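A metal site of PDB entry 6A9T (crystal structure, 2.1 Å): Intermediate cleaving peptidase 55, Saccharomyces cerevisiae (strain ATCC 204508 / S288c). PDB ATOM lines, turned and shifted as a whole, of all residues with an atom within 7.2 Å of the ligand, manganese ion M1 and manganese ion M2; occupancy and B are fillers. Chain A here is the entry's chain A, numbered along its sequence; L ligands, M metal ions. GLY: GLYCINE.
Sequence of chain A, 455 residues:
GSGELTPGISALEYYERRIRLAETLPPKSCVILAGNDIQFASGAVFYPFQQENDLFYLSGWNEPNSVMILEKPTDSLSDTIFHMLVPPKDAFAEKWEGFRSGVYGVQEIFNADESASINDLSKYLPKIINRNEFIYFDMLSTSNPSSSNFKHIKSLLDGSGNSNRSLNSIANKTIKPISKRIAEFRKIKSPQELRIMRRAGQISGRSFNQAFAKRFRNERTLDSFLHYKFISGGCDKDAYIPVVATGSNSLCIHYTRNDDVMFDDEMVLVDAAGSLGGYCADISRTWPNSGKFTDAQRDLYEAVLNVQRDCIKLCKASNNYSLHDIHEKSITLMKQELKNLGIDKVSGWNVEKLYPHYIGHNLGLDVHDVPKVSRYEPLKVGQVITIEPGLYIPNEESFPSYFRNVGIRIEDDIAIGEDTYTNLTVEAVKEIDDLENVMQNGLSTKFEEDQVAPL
Manganese ion M2 is bound by the side-chain carboxylate (OD1) of Asp 282 (2.1 Å), the side-chain carboxylate (OE1) of Glu 411 (2.2 Å), an oxygen (OXT) of the ligand (2.3 Å), the side-chain carboxylate (OD2) of Asp 271 (2.3 Å), the side-chain carboxylate (OD1) of Asp 271 (2.3 Å) and a nitrogen (N) of the ligand (2.5 Å).
Residues that only touch manganese ion M1: Thr 386.
Within 4 Å of manganese ion M1: Asp 282, His 361, Thr 386, Glu 388 and Glu 411.
Residues that only touch manganese ion M2: Tyr 240 (3.7 Å) and Ser 284 (3.6 Å).
Five residues have an atom within 4 Å of manganese ion M2: Tyr 240, Asp 271, Asp 282, Ser 284 and Glu 411.
Along chain A the residues within 4 Å of manganese ion M2 span positions 240 to 411.
Manganese ion M1 is bound by OE2 of Glu 411 (2.1 Å), O of the ligand (2.2 Å), OD2 of Asp 282 (2.2 Å), NE2 of His 361 (2.2 Å), OXT of the ligand (2.3 Å) and OE1 of Glu 388 (2.4 Å).
Manganese ion M1 has six donor atoms within binding distance.
NE2 of His 368 lies close to O of the ligand (2.9 Å).
Residues that only touch the ligand: Tyr 240.
Hydrophobic or aromatic side chains that line the ligand: Tyr 240, His 361 and His 368.
Within 4 Å of the ligand: Tyr 240, Asp 271, Asp 282, His 361, His 368, Glu 388 and Glu 411.
The nearest printed residue that does not touch the ligand is Val 367 (4.4 Å).
The backbone NH (N) of Glu 411 is in hydrogen-bond range of the backbone carbonyl oxygen (O) of Ser 284, 3.0 Å away.
The side-chain carboxylate (OD1) of Asp 282 sits close to the side-chain hydroxyl (OH) of Tyr 240, 2.8 Å away.
The side-chain carboxylate of Asp 271 sits close to the side-chain hydroxyl of Tyr 240.
The side-chain carboxylate of Asp 271 sits close to the guanidinium group of Arg 409 (2.9 Å).
The backbone carbonyl oxygen of Asp 271 sits at hydrogen-bond distance from the backbone NH of Val 243 (2.8 Å).
The side-chain hydroxyl (OG1) of Thr 386 lies close to the side-chain carboxylate (OE1) of Glu 388.
OE2 of Glu 388 lies within salt-bridge range of NE of Arg 409 (3.7 Å).
OH of Tyr 240 sits at hydrogen-bond distance from N of Ala 273, 3.5 Å away.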
ATOM      1  N   TYR A 240      30.673   2.306 -30.386  1.00  0.00           N
ATOM      2  CA  TYR A 240      31.579   3.304 -29.835  1.00  0.00           C
ATOM      3  C   TYR A 240      32.078   2.794 -28.496  1.00  0.00           C
ATOM      4  O   TYR A 240      31.587   1.789 -27.964  1.00  0.00           O
ATOM      5  CB  TYR A 240      30.874   4.663 -29.687  1.00  0.00           C
ATOM      6  CG  TYR A 240      29.515   4.577 -29.040  1.00  0.00           C
ATOM      7  CD1 TYR A 240      28.371   4.401 -29.814  1.00  0.00           C
ATOM      8  CD2 TYR A 240      29.362   4.668 -27.659  1.00  0.00           C
ATOM      9  CE1 TYR A 240      27.119   4.314 -29.233  1.00  0.00           C
ATOM     10  CE2 TYR A 240      28.113   4.582 -27.069  1.00  0.00           C
ATOM     11  CZ  TYR A 240      26.993   4.400 -27.861  1.00  0.00           C
ATOM     12  OH  TYR A 240      25.749   4.319 -27.282  1.00  0.00           O
ATOM     13  N   ILE A 241      33.060   3.487 -27.943  1.00  0.00           N
ATOM     14  CA  ILE A 241      33.594   3.165 -26.617  1.00  0.00           C
ATOM     15  C   ILE A 241      32.500   3.454 -25.592  1.00  0.00           C
ATOM     16  O   ILE A 241      31.995   4.582 -25.523  1.00  0.00           O
ATOM     17  CB  ILE A 241      34.882   3.935 -26.309  1.00  0.00           C
ATOM     18  CG1 ILE A 241      36.008   3.485 -27.240  1.00  0.00           C
ATOM     19  CG2 ILE A 241      35.280   3.749 -24.860  1.00  0.00           C
ATOM     20  CD1 ILE A 241      37.329   4.162 -26.994  1.00  0.00           C
ATOM     21  N   PRO A 242      32.093   2.467 -24.793  1.00  0.00           N
ATOM     22  CA  PRO A 242      30.907   2.635 -23.958  1.00  0.00           C
ATOM     23  C   PRO A 242      31.180   3.410 -22.679  1.00  0.00           C
ATOM     24  O   PRO A 242      32.291   3.429 -22.150  1.00  0.00           O
ATOM     25  CB  PRO A 242      30.502   1.183 -23.643  1.00  0.00           C
ATOM     26  CG  PRO A 242      31.812   0.448 -23.636  1.00  0.00           C
ATOM     27  CD  PRO A 242      32.661   1.104 -24.696  1.00  0.00           C
ATOM     28  N   VAL A 243      30.122   4.049 -22.195  1.00  0.00           N
ATOM     29  CA  VAL A 243      30.136   4.732 -20.907  1.00  0.00           C
ATOM     30  C   VAL A 243      29.338   3.899 -19.927  1.00  0.00           C
ATOM     31  O   VAL A 243      28.165   3.592 -20.180  1.00  0.00           O
ATOM     32  CB  VAL A 243      29.557   6.151 -21.018  1.00  0.00           C
ATOM     33  CG1 VAL A 243      29.475   6.817 -19.645  1.00  0.00           C
ATOM     34  CG2 VAL A 243      30.386   6.992 -21.977  1.00  0.00           C
ATOM     35  N   VAL A 270      24.545   4.592 -18.472  1.00  0.00           N
ATOM     36  CA  VAL A 270      25.175   3.722 -19.458  1.00  0.00           C
ATOM     37  C   VAL A 270      24.890   4.271 -20.849  1.00  0.00           C
ATOM     38  O   VAL A 270      23.724   4.433 -21.234  1.00  0.00           O
ATOM     39  CB  VAL A 270      24.705   2.269 -19.334  1.00  0.00           C
ATOM     40  CG1 VAL A 270      25.279   1.439 -20.475  1.00  0.00           C
ATOM     41  CG2 VAL A 270      25.123   1.688 -18.003  1.00  0.00           C
ATOM     42  N   ASP A 271      25.960   4.555 -21.596  1.00  0.00           N
ATOM     43  CA  ASP A 271      25.883   4.934 -23.002  1.00  0.00           C
ATOM     44  C   ASP A 271      26.620   3.872 -23.798  1.00  0.00           C
ATOM     45  O   ASP A 271      27.859   3.845 -23.791  1.00  0.00           O
ATOM     46  CB  ASP A 271      26.468   6.321 -23.229  1.00  0.00           C
ATOM     47  CG  ASP A 271      26.083   6.917 -24.583  1.00  0.00           C
ATOM     48  OD1 ASP A 271      25.688   6.145 -25.474  1.00  0.00           O
ATOM     49  OD2 ASP A 271      26.177   8.149 -24.740  1.00  0.00           O
ATOM     50  N   ALA A 272      25.881   2.997 -24.460  1.00  0.00           N
ATOM     51  CA  ALA A 272      26.484   1.878 -25.175  1.00  0.00           C
ATOM     52  C   ALA A 272      25.498   1.348 -26.201  1.00  0.00           C
ATOM     53  O   ALA A 272      24.283   1.406 -25.997  1.00  0.00           O
ATOM     54  CB  ALA A 272      26.898   0.763 -24.212  1.00  0.00           C
ATOM     55  N   ALA A 273      26.031   0.832 -27.303  1.00  0.00           N
ATOM     56  CA  ALA A 273      25.208   0.277 -28.368  1.00  0.00           C
ATOM     57  C   ALA A 273      26.101  -0.503 -29.322  1.00  0.00           C
ATOM     58  O   ALA A 273      27.315  -0.319 -29.363  1.00  0.00           O
ATOM     59  CB  ALA A 273      24.447   1.376 -29.133  1.00  0.00           C
ATOM     60  N   ALA A 281      23.993   2.044 -33.835  1.00  0.00           N
ATOM     61  CA  ALA A 281      22.968   2.495 -32.915  1.00  0.00           C
ATOM     62  C   ALA A 281      23.649   3.329 -31.828  1.00  0.00           C
ATOM     63  O   ALA A 281      24.877   3.439 -31.781  1.00  0.00           O
ATOM     64  CB  ALA A 281      22.209   1.300 -32.328  1.00  0.00           C
ATOM     65  N   ASP A 282      22.843   3.921 -30.953  1.00  0.00           N
ATOM     66  CA  ASP A 282      23.381   4.806 -29.922  1.00  0.00           C
ATOM     67  C   ASP A 282      22.338   4.976 -28.836  1.00  0.00           C
ATOM     68  O   ASP A 282      21.321   5.650 -29.055  1.00  0.00           O
ATOM     69  CB  ASP A 282      23.775   6.148 -30.536  1.00  0.00           C
ATOM     70  CG  ASP A 282      24.600   7.006 -29.604  1.00  0.00           C
ATOM     71  OD1 ASP A 282      24.765   6.631 -28.428  1.00  0.00           O
ATOM     72  OD2 ASP A 282      25.092   8.066 -30.058  1.00  0.00           O
ATOM     73  N   ILE A 283      22.567   4.375 -27.674  1.00  0.00           N
ATOM     74  CA  ILE A 283      21.576   4.335 -26.601  1.00  0.00           C
ATOM     75  C   ILE A 283      22.210   4.825 -25.309  1.00  0.00           C
ATOM     76  O   ILE A 283      23.348   4.450 -24.974  1.00  0.00           O
ATOM     77  CB  ILE A 283      20.997   2.919 -26.414  1.00  0.00           C
ATOM     78  CG1 ILE A 283      20.314   2.443 -27.702  1.00  0.00           C
ATOM     79  CG2 ILE A 283      20.009   2.885 -25.258  1.00  0.00           C
ATOM     80  CD1 ILE A 283      19.693   1.079 -27.582  1.00  0.00           C
ATOM     81  N   SER A 284      21.476   5.647 -24.570  1.00  0.00           N
ATOM     82  CA  SER A 284      21.812   5.996 -23.197  1.00  0.00           C
ATOM     83  C   SER A 284      20.608   5.685 -22.309  1.00  0.00           C
ATOM     84  O   SER A 284      19.484   6.069 -22.628  1.00  0.00           O
ATOM     85  CB  SER A 284      22.188   7.474 -23.051  1.00  0.00           C
ATOM     86  OG  SER A 284      23.302   7.799 -23.871  1.00  0.00           O
ATOM     87  N   ILE A 359      21.712  18.463 -28.023  1.00  0.00           N
ATOM     88  CA  ILE A 359      20.547  17.585 -27.914  1.00  0.00           C
ATOM     89  C   ILE A 359      20.798  16.257 -28.617  1.00  0.00           C
ATOM     90  O   ILE A 359      20.219  15.230 -28.245  1.00  0.00           O
ATOM     91  CB  ILE A 359      19.296  18.287 -28.453  1.00  0.00           C
ATOM     92  CG1 ILE A 359      18.035  17.466 -28.150  1.00  0.00           C
ATOM     93  CG2 ILE A 359      19.401  18.499 -29.960  1.00  0.00           C
ATOM     94  CD1 ILE A 359      17.894  17.084 -26.696  1.00  0.00           C
ATOM     95  N   GLY A 360      21.639  16.256 -29.648  1.00  0.00           N
ATOM     96  CA  GLY A 360      21.853  15.031 -30.405  1.00  0.00           C
ATOM     97  C   GLY A 360      22.683  15.309 -31.645  1.00  0.00           C
ATOM     98  O   GLY A 360      23.376  16.323 -31.735  1.00  0.00           O
ATOM     99  N   HIS A 361      22.597  14.384 -32.595  1.00  0.00           N
ATOM    100  CA  HIS A 361      23.475  14.387 -33.755  1.00  0.00           C
ATOM    101  C   HIS A 361      22.922  13.404 -34.781  1.00  0.00           C
ATOM    102  O   HIS A 361      22.165  12.487 -34.438  1.00  0.00           O
ATOM    103  CB  HIS A 361      24.904  13.995 -33.363  1.00  0.00           C
ATOM    104  CG  HIS A 361      24.990  12.714 -32.602  1.00  0.00           C
ATOM    105  ND1 HIS A 361      25.005  11.476 -33.220  1.00  0.00           N
ATOM    106  CD2 HIS A 361      25.028  12.464 -31.274  1.00  0.00           C
ATOM    107  CE1 HIS A 361      25.075  10.538 -32.305  1.00  0.00           C
ATOM    108  NE2 HIS A 361      25.087  11.107 -31.109  1.00  0.00           N
ATOM    109  N   ASN A 362      23.309  13.608 -36.039  1.00  0.00           N
ATOM    110  CA  ASN A 362      23.017  12.616 -37.063  1.00  0.00           C
ATOM    111  C   ASN A 362      23.722  11.302 -36.740  1.00  0.00           C
ATOM    112  O   ASN A 362      24.774  11.278 -36.113  1.00  0.00           O
ATOM    113  CB  ASN A 362      23.463  13.125 -38.441  1.00  0.00           C
ATOM    114  CG  ASN A 362      22.492  14.125 -39.032  1.00  0.00           C
ATOM    115  OD1 ASN A 362      21.475  13.747 -39.622  1.00  0.00           O
ATOM    116  ND2 ASN A 362      22.804  15.408 -38.894  1.00  0.00           N
ATOM    117  N   LEU A 363      23.102  10.202 -37.181  1.00  0.00           N
ATOM    118  CA  LEU A 363      23.593   8.870 -36.862  1.00  0.00           C
ATOM    119  C   LEU A 363      23.566   8.011 -38.124  1.00  0.00           C
ATOM    120  O   LEU A 363      22.589   8.029 -38.870  1.00  0.00           O
ATOM    121  CB  LEU A 363      22.742   8.220 -35.760  1.00  0.00           C
ATOM    122  CG  LEU A 363      23.159   6.837 -35.263  1.00  0.00           C
ATOM    123  CD1 LEU A 363      24.441   6.910 -34.446  1.00  0.00           C
ATOM    124  CD2 LEU A 363      22.040   6.224 -34.450  1.00  0.00           C
ATOM    125  N   VAL A 367      29.110   7.276 -35.724  1.00  0.00           N
ATOM    126  CA  VAL A 367      28.259   7.605 -34.581  1.00  0.00           C
ATOM    127  C   VAL A 367      27.824   9.063 -34.659  1.00  0.00           C
ATOM    128  O   VAL A 367      26.627   9.382 -34.662  1.00  0.00           O
ATOM    129  CB  VAL A 367      28.984   7.311 -33.257  1.00  0.00           C
ATOM    130  CG1 VAL A 367      28.068   7.575 -32.075  1.00  0.00           C
ATOM    131  CG2 VAL A 367      29.471   5.874 -33.240  1.00  0.00           C
ATOM    132  N   HIS A 368      28.796   9.969 -34.731  1.00  0.00           N
ATOM    133  CA  HIS A 368      28.523  11.372 -35.034  1.00  0.00           C
ATOM    134  C   HIS A 368      28.585  11.530 -36.552  1.00  0.00           C
ATOM    135  O   HIS A 368      29.560  12.011 -37.124  1.00  0.00           O
ATOM    136  CB  HIS A 368      29.491  12.283 -34.301  1.00  0.00           C
ATOM    137  CG  HIS A 368      29.330  12.255 -32.809  1.00  0.00           C
ATOM    138  ND1 HIS A 368      30.185  12.918 -31.947  1.00  0.00           N
ATOM    139  CD2 HIS A 368      28.405  11.650 -32.027  1.00  0.00           C
ATOM    140  CE1 HIS A 368      29.792  12.712 -30.708  1.00  0.00           C
ATOM    141  NE2 HIS A 368      28.718  11.941 -30.725  1.00  0.00           N
ATOM    142  N   THR A 386      19.832  11.499 -33.011  1.00  0.00           N
ATOM    143  CA  THR A 386      19.630  11.105 -31.630  1.00  0.00           C
ATOM    144  C   THR A 386      18.963  12.247 -30.866  1.00  0.00           C
ATOM    145  O   THR A 386      19.104  13.423 -31.211  1.00  0.00           O
ATOM    146  CB  THR A 386      20.959  10.745 -30.967  1.00  0.00           C
ATOM    147  OG1 THR A 386      21.807  11.895 -30.912  1.00  0.00           O
ATOM    148  CG2 THR A 386      21.661   9.642 -31.736  1.00  0.00           C
ATOM    149  N   ILE A 387      18.213  11.878 -29.831  1.00  0.00           N
ATOM    150  CA  ILE A 387      17.627  12.822 -28.889  1.00  0.00           C
ATOM    151  C   ILE A 387      18.090  12.393 -27.517  1.00  0.00           C
ATOM    152  O   ILE A 387      17.605  11.380 -26.986  1.00  0.00           O
ATOM    153  CB  ILE A 387      16.097  12.857 -28.973  1.00  0.00           C
ATOM    154  CG1 ILE A 387      15.639  13.243 -30.384  1.00  0.00           C
ATOM    155  CG2 ILE A 387      15.532  13.832 -27.958  1.00  0.00           C
ATOM    156  CD1 ILE A 387      15.986  14.662 -30.772  1.00  0.00           C
ATOM    157  N   GLU A 388      19.027  13.148 -26.925  1.00  0.00           N
ATOM    158  CA  GLU A 388      19.725  12.710 -25.712  1.00  0.00           C
ATOM    159  C   GLU A 388      19.959  13.882 -24.776  1.00  0.00           C
ATOM    160  O   GLU A 388      21.102  14.279 -24.524  1.00  0.00           O
ATOM    161  CB  GLU A 388      21.034  12.031 -26.082  1.00  0.00           C
ATOM    162  CG  GLU A 388      21.863  12.781 -27.115  1.00  0.00           C
ATOM    163  CD  GLU A 388      23.203  12.134 -27.351  1.00  0.00           C
ATOM    164  OE1 GLU A 388      23.617  12.037 -28.529  1.00  0.00           O
ATOM    165  OE2 GLU A 388      23.841  11.704 -26.362  1.00  0.00           O
ATOM    166  N   ARG A 409      21.152  10.612 -18.392  1.00  0.00           N
ATOM    167  CA  ARG A 409      20.962  10.835 -19.816  1.00  0.00           C
ATOM    168  C   ARG A 409      20.075   9.727 -20.371  1.00  0.00           C
ATOM    169  O   ARG A 409      20.213   8.566 -20.001  1.00  0.00           O
ATOM    170  CB  ARG A 409      22.285  10.884 -20.585  1.00  0.00           C
ATOM    171  CG  ARG A 409      22.100  11.192 -22.063  1.00  0.00           C
ATOM    172  CD  ARG A 409      23.364  11.697 -22.731  1.00  0.00           C
ATOM    173  NE  ARG A 409      24.393  10.671 -22.853  1.00  0.00           N
ATOM    174  CZ  ARG A 409      25.480  10.621 -22.096  1.00  0.00           C
ATOM    175  NH1 ARG A 409      25.694  11.542 -21.166  1.00  0.00           N
ATOM    176  NH2 ARG A 409      26.369   9.648 -22.265  1.00  0.00           N
ATOM    177  N   GLU A 411      18.810   8.491 -24.172  1.00  0.00           N
ATOM    178  CA  GLU A 411      19.094   8.675 -25.585  1.00  0.00           C
ATOM    179  C   GLU A 411      18.378   7.625 -26.424  1.00  0.00           C
ATOM    180  O   GLU A 411      18.385   6.445 -26.084  1.00  0.00           O
ATOM    181  CB  GLU A 411      20.600   8.601 -25.859  1.00  0.00           C
ATOM    182  CG  GLU A 411      20.986   8.678 -27.324  1.00  0.00           C
ATOM    183  CD  GLU A 411      22.484   8.790 -27.522  1.00  0.00           C
ATOM    184  OE1 GLU A 411      23.240   8.392 -26.607  1.00  0.00           O
ATOM    185  OE2 GLU A 411      22.903   9.280 -28.582  1.00  0.00           O
ATOM    186  N   ASP A 412      17.777   8.070 -27.521  1.00  0.00           N
ATOM    187  CA  ASP A 412      17.145   7.184 -28.491  1.00  0.00           C
ATOM    188  C   ASP A 412      17.482   7.666 -29.894  1.00  0.00           C
ATOM    189  O   ASP A 412      17.856   8.822 -30.100  1.00  0.00           O
ATOM    190  CB  ASP A 412      15.619   7.126 -28.291  1.00  0.00           C
ATOM    191  CG  ASP A 412      15.224   6.312 -27.073  1.00  0.00           C
ATOM    192  OD1 ASP A 412      15.352   5.066 -27.112  1.00  0.00           O
ATOM    193  OD2 ASP A 412      14.805   6.909 -26.059  1.00  0.00           O
ATOM    194  N   ASP A 413      17.351   6.759 -30.853  1.00  0.00           N
ATOM    195  CA  ASP A 413      17.668   7.028 -32.255  1.00  0.00           C
ATOM    196  C   ASP A 413      16.358   7.190 -33.017  1.00  0.00           C
ATOM    197  O   ASP A 413      15.541   6.261 -33.067  1.00  0.00           O
ATOM    198  CB  ASP A 413      18.513   5.908 -32.836  1.00  0.00           C
ATOM    199  CG  ASP A 413      19.748   5.622 -32.004  1.00  0.00           C
ATOM    200  OD1 ASP A 413      20.199   6.544 -31.307  1.00  0.00           O
ATOM    201  OD2 ASP A 413      20.257   4.481 -32.051  1.00  0.00           O
HETATM  202  N   GLY L   1      27.645   7.798 -27.717  1.00  0.00           N
HETATM  203  CA  GLY L   1      28.019   9.196 -27.856  1.00  0.00           C
HETATM  204  C   GLY L   1      26.823  10.114 -27.984  1.00  0.00           C
HETATM  205  O   GLY L   1      26.759  10.921 -28.906  1.00  0.00           O
HETATM  206  OXT GLY L   1      25.905  10.083 -27.168  1.00  0.00           O
HETATM  207 MN    MN M   1      24.779  10.083 -29.143  1.00  0.00          MN
HETATM  208 MN    MN M   2      25.338   7.925 -26.833  1.00  0.00          MN
